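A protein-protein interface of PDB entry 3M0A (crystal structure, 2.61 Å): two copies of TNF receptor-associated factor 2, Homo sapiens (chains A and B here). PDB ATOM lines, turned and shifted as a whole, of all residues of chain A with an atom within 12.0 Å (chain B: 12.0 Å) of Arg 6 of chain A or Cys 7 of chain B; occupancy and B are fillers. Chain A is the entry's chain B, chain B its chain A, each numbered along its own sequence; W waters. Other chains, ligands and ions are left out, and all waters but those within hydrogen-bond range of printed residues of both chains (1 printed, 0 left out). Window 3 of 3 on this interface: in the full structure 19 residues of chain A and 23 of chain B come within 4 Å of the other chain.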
ATOM      1  N   GLU A   2     -35.460  -5.673   3.206  1.00  0.00           N
ATOM      2  CA  GLU A   2     -34.219  -6.502   3.219  1.00  0.00           C
ATOM      3  C   GLU A   2     -33.210  -6.041   4.318  1.00  0.00           C
ATOM      4  O   GLU A   2     -33.544  -6.048   5.506  1.00  0.00           O
ATOM      5  CB  GLU A   2     -33.550  -6.543   1.831  1.00  0.00           C
ATOM      6  CG  GLU A   2     -33.984  -7.653   0.843  1.00  0.00           C
ATOM      7  CD  GLU A   2     -33.102  -7.660  -0.452  1.00  0.00           C
ATOM      8  OE1 GLU A   2     -32.037  -8.335  -0.450  1.00  0.00           O
ATOM      9  OE2 GLU A   2     -33.472  -6.987  -1.462  1.00  0.00           O
ATOM     10  N   LEU A   3     -32.004  -5.621   3.922  1.00  0.00           N
ATOM     11  CA  LEU A   3     -30.846  -5.576   4.816  1.00  0.00           C
ATOM     12  C   LEU A   3     -31.019  -5.205   6.281  1.00  0.00           C
ATOM     13  O   LEU A   3     -30.434  -5.843   7.140  1.00  0.00           O
ATOM     14  CB  LEU A   3     -29.729  -4.755   4.218  1.00  0.00           C
ATOM     15  CG  LEU A   3     -28.382  -5.129   4.793  1.00  0.00           C
ATOM     16  CD1 LEU A   3     -28.143  -6.633   4.572  1.00  0.00           C
ATOM     17  CD2 LEU A   3     -27.281  -4.318   4.162  1.00  0.00           C
ATOM     18  N   LEU A   4     -31.807  -4.185   6.563  1.00  0.00           N
ATOM     19  CA  LEU A   4     -31.975  -3.677   7.931  1.00  0.00           C
ATOM     20  C   LEU A   4     -32.906  -4.507   8.841  1.00  0.00           C
ATOM     21  O   LEU A   4     -32.743  -4.486  10.077  1.00  0.00           O
ATOM     22  CB  LEU A   4     -32.520  -2.244   7.870  1.00  0.00           C
ATOM     23  CG  LEU A   4     -32.292  -1.302   9.057  1.00  0.00           C
ATOM     24  CD1 LEU A   4     -30.902  -0.648   8.927  1.00  0.00           C
ATOM     25  CD2 LEU A   4     -33.369  -0.203   9.162  1.00  0.00           C
ATOM     26  N   GLN A   5     -33.922  -5.151   8.242  1.00  0.00           N
ATOM     27  CA  GLN A   5     -34.844  -6.061   8.961  1.00  0.00           C
ATOM     28  C   GLN A   5     -34.257  -7.522   9.020  1.00  0.00           C
ATOM     29  O   GLN A   5     -34.337  -8.198  10.065  1.00  0.00           O
ATOM     30  CB  GLN A   5     -36.269  -6.010   8.389  1.00  0.00           C
ATOM     31  N   ARG A   6     -33.650  -7.949   7.903  1.00  0.00           N
ATOM     32  CA  ARG A   6     -32.928  -9.177   7.775  1.00  0.00           C
ATOM     33  C   ARG A   6     -31.796  -9.130   8.777  1.00  0.00           C
ATOM     34  O   ARG A   6     -31.406 -10.147   9.395  1.00  0.00           O
ATOM     35  CB  ARG A   6     -32.386  -9.262   6.374  1.00  0.00           C
ATOM     36  CG  ARG A   6     -31.557 -10.453   6.136  1.00  0.00           C
ATOM     37  CD  ARG A   6     -30.805 -10.332   4.852  1.00  0.00           C
ATOM     38  NE  ARG A   6     -31.649 -10.417   3.670  1.00  0.00           N
ATOM     39  CZ  ARG A   6     -31.245 -10.931   2.509  1.00  0.00           C
ATOM     40  NH1 ARG A   6     -30.010 -11.421   2.403  1.00  0.00           N
ATOM     41  NH2 ARG A   6     -32.072 -10.974   1.457  1.00  0.00           N
ATOM     42  N   CYS A   7     -31.299  -7.928   8.997  1.00  0.00           N
ATOM     43  CA  CYS A   7     -30.292  -7.778  10.005  1.00  0.00           C
ATOM     44  C   CYS A   7     -30.842  -7.813  11.436  1.00  0.00           C
ATOM     45  O   CYS A   7     -30.226  -8.415  12.312  1.00  0.00           O
ATOM     46  CB  CYS A   7     -29.477  -6.542   9.747  1.00  0.00           C
ATOM     47  SG  CYS A   7     -28.297  -6.359  11.018  1.00  0.00           S
ATOM     48  N   GLU A   8     -32.003  -7.197  11.684  1.00  0.00           N
ATOM     49  CA  GLU A   8     -32.603  -7.185  13.072  1.00  0.00           C
ATOM     50  C   GLU A   8     -33.004  -8.593  13.522  1.00  0.00           C
ATOM     51  O   GLU A   8     -33.005  -8.930  14.724  1.00  0.00           O
ATOM     52  CB  GLU A   8     -33.806  -6.230  13.210  1.00  0.00           C
ATOM     53  N   SER A   9     -33.375  -9.393  12.530  1.00  0.00           N
ATOM     54  CA  SER A   9     -33.700 -10.793  12.703  1.00  0.00           C
ATOM     55  C   SER A   9     -32.448 -11.554  13.219  1.00  0.00           C
ATOM     56  O   SER A   9     -32.511 -12.213  14.255  1.00  0.00           O
ATOM     57  CB  SER A   9     -34.213 -11.342  11.380  1.00  0.00           C
ATOM     58  OG  SER A   9     -34.778 -12.607  11.577  1.00  0.00           O
ATOM     59  N   LEU A  10     -31.311 -11.392  12.534  1.00  0.00           N
ATOM     60  CA  LEU A  10     -30.036 -11.897  13.020  1.00  0.00           C
ATOM     61  C   LEU A  10     -29.667 -11.528  14.446  1.00  0.00           C
ATOM     62  O   LEU A  10     -28.981 -12.283  15.120  1.00  0.00           O
ATOM     63  CB  LEU A  10     -28.907 -11.518  12.097  1.00  0.00           C
ATOM     64  CG  LEU A  10     -28.909 -12.270  10.765  1.00  0.00           C
ATOM     65  CD1 LEU A  10     -27.762 -11.768   9.857  1.00  0.00           C
ATOM     66  CD2 LEU A  10     -28.914 -13.800  10.919  1.00  0.00           C
ATOM     67  N   GLU A  11     -30.118 -10.373  14.910  1.00  0.00           N
ATOM     68  CA  GLU A  11     -29.981 -10.000  16.330  1.00  0.00           C
ATOM     69  C   GLU A  11     -30.947 -10.728  17.280  1.00  0.00           C
ATOM     70  O   GLU A  11     -30.450 -11.376  18.230  1.00  0.00           O
ATOM     71  CB  GLU A  11     -29.986  -8.482  16.536  1.00  0.00           C
ATOM     72  CG  GLU A  11     -28.573  -7.893  16.329  1.00  0.00           C
ATOM     73  CD  GLU A  11     -28.540  -6.375  16.008  1.00  0.00           C
ATOM     74  OE1 GLU A  11     -27.405  -5.866  15.719  1.00  0.00           O
ATOM     75  OE2 GLU A  11     -29.631  -5.718  16.042  1.00  0.00           O
ATOM     76  N   LYS A  12     -32.271 -10.681  17.037  1.00  0.00           N
ATOM     77  CA  LYS A  12     -33.230 -11.465  17.853  1.00  0.00           C
ATOM     78  C   LYS A  12     -32.703 -12.916  18.073  1.00  0.00           C
ATOM     79  O   LYS A  12     -32.426 -13.333  19.220  1.00  0.00           O
ATOM     80  CB  LYS A  12     -34.672 -11.442  17.265  1.00  0.00           C
ATOM     81  N   LYS A  13     -32.537 -13.665  16.977  1.00  0.00           N
ATOM     82  CA  LYS A  13     -32.083 -15.057  17.034  1.00  0.00           C
ATOM     83  C   LYS A  13     -30.734 -15.166  17.748  1.00  0.00           C
ATOM     84  O   LYS A  13     -30.637 -15.873  18.763  1.00  0.00           O
ATOM     85  CB  LYS A  13     -32.039 -15.743  15.642  1.00  0.00           C
ATOM     86  N   THR A  14     -29.713 -14.449  17.276  1.00  0.00           N
ATOM     87  CA  THR A  14     -28.366 -14.618  17.818  1.00  0.00           C
ATOM     88  C   THR A  14     -28.387 -14.404  19.322  1.00  0.00           C
ATOM     89  O   THR A  14     -27.517 -14.872  20.044  1.00  0.00           O
ATOM     90  CB  THR A  14     -27.443 -13.626  17.202  1.00  0.00           C
ATOM     91  OG1 THR A  14     -27.049 -14.113  15.920  1.00  0.00           O
ATOM     92  CG2 THR A  14     -26.225 -13.453  18.028  1.00  0.00           C
ATOM     93  N   ALA A  15     -29.410 -13.708  19.794  1.00  0.00           N
ATOM     94  CA  ALA A  15     -29.491 -13.372  21.194  1.00  0.00           C
ATOM     95  C   ALA A  15     -30.015 -14.560  21.961  1.00  0.00           C
ATOM     96  O   ALA A  15     -29.596 -14.789  23.092  1.00  0.00           O
ATOM     97  CB  ALA A  15     -30.379 -12.155  21.412  1.00  0.00           C
ATOM     98  N   PHE A  17     -29.285 -17.496  21.301  1.00  0.00           N
ATOM     99  CA  PHE A  17     -28.160 -18.480  21.308  1.00  0.00           C
ATOM    100  C   PHE A  17     -27.363 -18.460  22.583  1.00  0.00           C
ATOM    101  O   PHE A  17     -26.983 -19.522  23.074  1.00  0.00           O
ATOM    102  CB  PHE A  17     -27.175 -18.202  20.203  1.00  0.00           C
ATOM    103  CG  PHE A  17     -27.698 -18.513  18.838  1.00  0.00           C
ATOM    104  CD1 PHE A  17     -28.928 -19.181  18.682  1.00  0.00           C
ATOM    105  CD2 PHE A  17     -26.931 -18.208  17.701  1.00  0.00           C
ATOM    106  CE1 PHE A  17     -29.417 -19.516  17.400  1.00  0.00           C
ATOM    107  CE2 PHE A  17     -27.406 -18.505  16.431  1.00  0.00           C
ATOM    108  CZ  PHE A  17     -28.672 -19.169  16.272  1.00  0.00           C
ATOM    109  N   GLU B   2     -19.955  -7.492   0.077  1.00  0.00           N
ATOM    110  CA  GLU B   2     -19.783  -7.017   1.483  1.00  0.00           C
ATOM    111  C   GLU B   2     -21.109  -7.109   2.218  1.00  0.00           C
ATOM    112  O   GLU B   2     -21.643  -8.202   2.332  1.00  0.00           O
ATOM    113  CB  GLU B   2     -19.183  -5.608   1.585  1.00  0.00           C
ATOM    114  CG  GLU B   2     -18.547  -5.303   2.950  1.00  0.00           C
ATOM    115  CD  GLU B   2     -17.600  -4.114   2.901  1.00  0.00           C
ATOM    116  OE1 GLU B   2     -17.960  -3.075   3.484  1.00  0.00           O
ATOM    117  OE2 GLU B   2     -16.511  -4.207   2.280  1.00  0.00           O
ATOM    118  N   LEU B   3     -21.664  -5.996   2.689  1.00  0.00           N
ATOM    119  CA  LEU B   3     -22.714  -6.082   3.703  1.00  0.00           C
ATOM    120  C   LEU B   3     -23.809  -7.146   3.527  1.00  0.00           C
ATOM    121  O   LEU B   3     -24.189  -7.779   4.503  1.00  0.00           O
ATOM    122  CB  LEU B   3     -23.323  -4.727   4.016  1.00  0.00           C
ATOM    123  CG  LEU B   3     -23.266  -4.482   5.520  1.00  0.00           C
ATOM    124  CD1 LEU B   3     -21.932  -3.853   5.928  1.00  0.00           C
ATOM    125  CD2 LEU B   3     -24.398  -3.610   5.928  1.00  0.00           C
ATOM    126  N   LEU B   4     -24.279  -7.375   2.303  1.00  0.00           N
ATOM    127  CA  LEU B   4     -25.367  -8.351   2.037  1.00  0.00           C
ATOM    128  C   LEU B   4     -24.931  -9.810   1.902  1.00  0.00           C
ATOM    129  O   LEU B   4     -25.725 -10.723   2.070  1.00  0.00           O
ATOM    130  CB  LEU B   4     -26.128  -7.969   0.772  1.00  0.00           C
ATOM    131  CG  LEU B   4     -26.875  -6.644   0.786  1.00  0.00           C
ATOM    132  CD1 LEU B   4     -26.746  -6.035  -0.581  1.00  0.00           C
ATOM    133  CD2 LEU B   4     -28.325  -6.810   1.164  1.00  0.00           C
ATOM    134  N   GLN B   5     -23.673 -10.004   1.546  1.00  0.00           N
ATOM    135  CA  GLN B   5     -23.053 -11.309   1.542  1.00  0.00           C
ATOM    136  C   GLN B   5     -22.768 -11.746   2.969  1.00  0.00           C
ATOM    137  O   GLN B   5     -22.899 -12.906   3.309  1.00  0.00           O
ATOM    138  CB  GLN B   5     -21.752 -11.255   0.733  1.00  0.00           C
ATOM    139  CG  GLN B   5     -21.972 -11.177  -0.778  1.00  0.00           C
ATOM    140  CD  GLN B   5     -22.097 -12.562  -1.424  1.00  0.00           C
ATOM    141  OE1 GLN B   5     -21.131 -13.059  -2.005  1.00  0.00           O
ATOM    142  NE2 GLN B   5     -23.279 -13.192  -1.313  1.00  0.00           N
ATOM    143  N   ARG B   6     -22.362 -10.790   3.787  1.00  0.00           N
ATOM    144  CA  ARG B   6     -22.062 -11.038   5.165  1.00  0.00           C
ATOM    145  C   ARG B   6     -23.332 -11.363   5.924  1.00  0.00           C
ATOM    146  O   ARG B   6     -23.295 -12.018   6.954  1.00  0.00           O
ATOM    147  CB  ARG B   6     -21.352  -9.840   5.778  1.00  0.00           C
ATOM    148  CG  ARG B   6     -19.899  -9.751   5.367  1.00  0.00           C
ATOM    149  CD  ARG B   6     -19.029  -9.169   6.469  1.00  0.00           C
ATOM    150  NE  ARG B   6     -18.769  -7.742   6.316  1.00  0.00           N
ATOM    151  CZ  ARG B   6     -18.039  -7.022   7.165  1.00  0.00           C
ATOM    152  NH1 ARG B   6     -17.511  -7.602   8.233  1.00  0.00           N
ATOM    153  NH2 ARG B   6     -17.843  -5.720   6.950  1.00  0.00           N
ATOM    154  N   CYS B   7     -24.451 -10.932   5.373  1.00  0.00           N
ATOM    155  CA  CYS B   7     -25.738 -11.096   5.990  1.00  0.00           C
ATOM    156  C   CYS B   7     -26.382 -12.429   5.595  1.00  0.00           C
ATOM    157  O   CYS B   7     -26.960 -13.136   6.441  1.00  0.00           O
ATOM    158  CB  CYS B   7     -26.612  -9.943   5.559  1.00  0.00           C
ATOM    159  SG  CYS B   7     -28.056  -9.847   6.487  1.00  0.00           S
ATOM    160  N   GLU B   8     -26.304 -12.744   4.306  1.00  0.00           N
ATOM    161  CA  GLU B   8     -26.666 -14.043   3.765  1.00  0.00           C
ATOM    162  C   GLU B   8     -25.945 -15.089   4.591  1.00  0.00           C
ATOM    163  O   GLU B   8     -26.589 -15.844   5.256  1.00  0.00           O
ATOM    164  CB  GLU B   8     -26.188 -14.148   2.319  1.00  0.00           C
ATOM    165  CG  GLU B   8     -27.068 -14.801   1.266  1.00  0.00           C
ATOM    166  CD  GLU B   8     -26.685 -14.284  -0.172  1.00  0.00           C
ATOM    167  OE1 GLU B   8     -26.841 -13.059  -0.478  1.00  0.00           O
ATOM    168  OE2 GLU B   8     -26.202 -15.103  -1.005  1.00  0.00           O
ATOM    169  N   SER B   9     -24.614 -15.096   4.584  1.00  0.00           N
ATOM    170  CA  SER B   9     -23.818 -16.114   5.257  1.00  0.00           C
ATOM    171  C   SER B   9     -24.101 -16.236   6.765  1.00  0.00           C
ATOM    172  O   SER B   9     -24.264 -17.357   7.301  1.00  0.00           O
ATOM    173  CB  SER B   9     -22.340 -15.863   5.028  1.00  0.00           C
ATOM    174  OG  SER B   9     -21.933 -14.733   5.777  1.00  0.00           O
ATOM    175  N   LEU B  10     -24.171 -15.094   7.438  1.00  0.00           N
ATOM    176  CA  LEU B  10     -24.548 -15.035   8.833  1.00  0.00           C
ATOM    177  C   LEU B  10     -25.867 -15.781   9.048  1.00  0.00           C
ATOM    178  O   LEU B  10     -25.991 -16.621   9.950  1.00  0.00           O
ATOM    179  CB  LEU B  10     -24.696 -13.584   9.249  1.00  0.00           C
ATOM    180  CG  LEU B  10     -24.094 -13.068  10.533  1.00  0.00           C
ATOM    181  CD1 LEU B  10     -22.691 -13.562  10.611  1.00  0.00           C
ATOM    182  CD2 LEU B  10     -24.165 -11.557  10.548  1.00  0.00           C
ATOM    183  N   GLU B  11     -26.837 -15.508   8.191  1.00  0.00           N
ATOM    184  CA  GLU B  11     -28.143 -16.102   8.359  1.00  0.00           C
ATOM    185  C   GLU B  11     -28.120 -17.596   8.035  1.00  0.00           C
ATOM    186  O   GLU B  11     -28.924 -18.361   8.614  1.00  0.00           O
ATOM    187  CB  GLU B  11     -29.247 -15.306   7.617  1.00  0.00           C
ATOM    188  CG  GLU B  11     -29.691 -15.830   6.235  1.00  0.00           C
ATOM    189  CD  GLU B  11     -30.118 -14.715   5.204  1.00  0.00           C
ATOM    190  OE1 GLU B  11     -30.413 -13.556   5.645  1.00  0.00           O
ATOM    191  OE2 GLU B  11     -30.177 -15.038   3.967  1.00  0.00           O
ATOM    192  N   LYS B  12     -27.185 -18.014   7.173  1.00  0.00           N
ATOM    193  CA  LYS B  12     -26.983 -19.448   6.841  1.00  0.00           C
ATOM    194  C   LYS B  12     -26.312 -20.235   7.981  1.00  0.00           C
ATOM    195  O   LYS B  12     -26.749 -21.339   8.334  1.00  0.00           O
ATOM    196  CB  LYS B  12     -26.173 -19.596   5.568  1.00  0.00           C
ATOM    197  CG  LYS B  12     -25.717 -20.994   5.239  1.00  0.00           C
ATOM    198  CD  LYS B  12     -25.526 -21.130   3.730  1.00  0.00           C
ATOM    199  CE  LYS B  12     -24.993 -22.494   3.284  1.00  0.00           C
ATOM    200  NZ  LYS B  12     -24.949 -22.644   1.790  1.00  0.00           N
ATOM    201  N   LYS B  13     -25.240 -19.648   8.528  1.00  0.00           N
ATOM    202  CA  LYS B  13     -24.538 -20.125   9.720  1.00  0.00           C
ATOM    203  C   LYS B  13     -25.532 -20.300  10.887  1.00  0.00           C
ATOM    204  O   LYS B  13     -25.643 -21.379  11.517  1.00  0.00           O
ATOM    205  CB  LYS B  13     -23.408 -19.123  10.096  1.00  0.00           C
ATOM    206  CG  LYS B  13     -22.015 -19.518   9.605  1.00  0.00           C
ATOM    207  CD  LYS B  13     -20.870 -18.742  10.250  1.00  0.00           C
ATOM    208  CE  LYS B  13     -20.318 -17.644   9.262  1.00  0.00           C
ATOM    209  NZ  LYS B  13     -19.769 -18.181   7.953  1.00  0.00           N
ATOM    210  N   THR B  14     -26.260 -19.220  11.124  1.00  0.00           N
ATOM    211  CA  THR B  14     -27.163 -19.094  12.213  1.00  0.00           C
ATOM    212  C   THR B  14     -28.220 -20.176  12.147  1.00  0.00           C
ATOM    213  O   THR B  14     -28.438 -20.883  13.132  1.00  0.00           O
ATOM    214  CB  THR B  14     -27.775 -17.683  12.182  1.00  0.00           C
ATOM    215  OG1 THR B  14     -26.874 -16.802  12.826  1.00  0.00           O
ATOM    216  CG2 THR B  14     -29.096 -17.602  12.947  1.00  0.00           C
ATOM    217  N   ALA B  15     -28.872 -20.309  10.996  1.00  0.00           N
ATOM    218  CA  ALA B  15     -29.918 -21.321  10.823  1.00  0.00           C
ATOM    219  C   ALA B  15     -29.427 -22.761  11.071  1.00  0.00           C
ATOM    220  O   ALA B  15     -30.186 -23.565  11.672  1.00  0.00           O
ATOM    221  CB  ALA B  15     -30.560 -21.229   9.452  1.00  0.00           C
ATOM    222  N   THR B  16     -28.192 -23.070  10.615  1.00  0.00           N
ATOM    223  CA  THR B  16     -27.605 -24.435  10.731  1.00  0.00           C
ATOM    224  C   THR B  16     -27.138 -24.713  12.161  1.00  0.00           C
ATOM    225  O   THR B  16     -27.329 -25.838  12.720  1.00  0.00           O
ATOM    226  CB  THR B  16     -26.378 -24.699   9.768  1.00  0.00           C
ATOM    227  OG1 THR B  16     -26.583 -24.102   8.492  1.00  0.00           O
ATOM    228  CG2 THR B  16     -26.190 -26.187   9.581  1.00  0.00           C
HETATM  229  O   HOH W   1     -28.361 -11.001   0.314  1.00  0.00           O
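The side-chain carboxylate (OE1) of Glu 11 of chain B lies within salt-bridge range of the guanidinium group (NH1) of Arg 6 of chain A (3.9 Å).
OG1 of Thr 14 of chain B sits at hydrogen-bond distance from O of Leu 10 of chain B (3.0 Å).
OE1 of Glu 2 of chain A is in salt-bridge range of NH2 of Arg 6 of chain A (3.3 Å).
The backbone carbonyl oxygen (O) of Leu 10 of chain A lies within hydrogen-bond range of the side-chain hydroxyl (OG1) of Thr 14 of chain A (2.8 Å).
Among the printed residues, pairs that only touch across the chains: Leu 3 of chain A with Leu 3 of chain B, Leu 3 of chain A with Leu 4 of chain B, Leu 3 of chain A with Cys 7 of chain B, Arg 6 of chain A with Cys 7 of chain B, Leu 10 of chain A with Cys 7 of chain B, Leu 10 of chain A with Leu 10 of chain B, Leu 10 of chain A with Glu 11 of chain B and Phe 17 of chain A with Thr 14 of chain B.
Arg 6 of chain A touches just these residues of chain B: Cys 7 and Glu 11.
Cys 7 of chain B touches just these residues of chain A: Leu 3, Arg 6 and Leu 10.
No residue of chain B comes within 4 Å of Glu 2 of chain A.
Leu 3 of chain A touches just these residues of chain B: Leu 3 (3.5 Å), Leu 4 (3.4 Å) and Cys 7 (3.7 Å).
Leu 4 of chain A touches none of the printed residues of chain B.
No residue of chain B comes within 4 Å of Ser 9 of chain A.
Of chain B, only Cys 7 (3.8 Å), Leu 10 (3.6 Å) and Glu 11 (3.5 Å) come within 4 Å of Leu 10 of chain A.
Leu 3 of chain B touches just one residue of chain A: Leu 3 (3.5 Å).
Of the printed residues of chain A, Leu 4 of chain B touches Leu 3 (3.4 Å).
No residue of chain A comes within 4 Å of Glu 8 of chain B.
Of the printed residues of chain A, Leu 10 of chain B touches Leu 10.
Of the printed residues of chain A, Thr 14 of chain B touches Phe 17 (3.6 Å).
Printed residues of chain B within 4 Å of Phe 17 of chain A: Thr 14.
Lys 13 of chain A touches none of the printed residues of chain B.
Gln 5 of chain B touches none of the printed residues of chain A.
The nearest printed residue of chain A that does not touch Thr 14 of chain B is Leu 10 of chain A (4.1 Å).
Of the 15 printed residues of chain A, 4 touch a printed residue of chain B.
Hydrophobic or aromatic side chains of chain A that line the printed part of chain B: Leu 3, Leu 10 and Phe 17.
Along chain A the printed residues that touch a printed residue of chain B span positions 3 to 17.
Leu 3 of chain B touches its own counterpart, Leu 3 of chain A.
Leu 3 of chain A touches Leu 4 of chain B, but with the chains exchanged Leu 4 of chain A does not touch Leu 3 of chain B (7.5 Å).
Arg 6 of chain A touches Cys 7 of chain B, but with the chains exchanged Cys 7 of chain A does not touch Arg 6 of chain B (8.6 Å).
Leu 10 of chain A touches Cys 7 of chain B, but with the chains exchanged Cys 7 of chain A does not touch Leu 10 of chain B (6.7 Å).
Of the 9 pairs that touch across the chains among the printed residues, 2 have their exchanged pair printed and touching as well.
Water W1 lies within hydrogen-bond range of OE1 of Glu 8 of chain B (2.7 Å), NH1 of Arg 6 of chain A (2.7 Å) and O of Leu 4 of chain B (3.2 Å).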
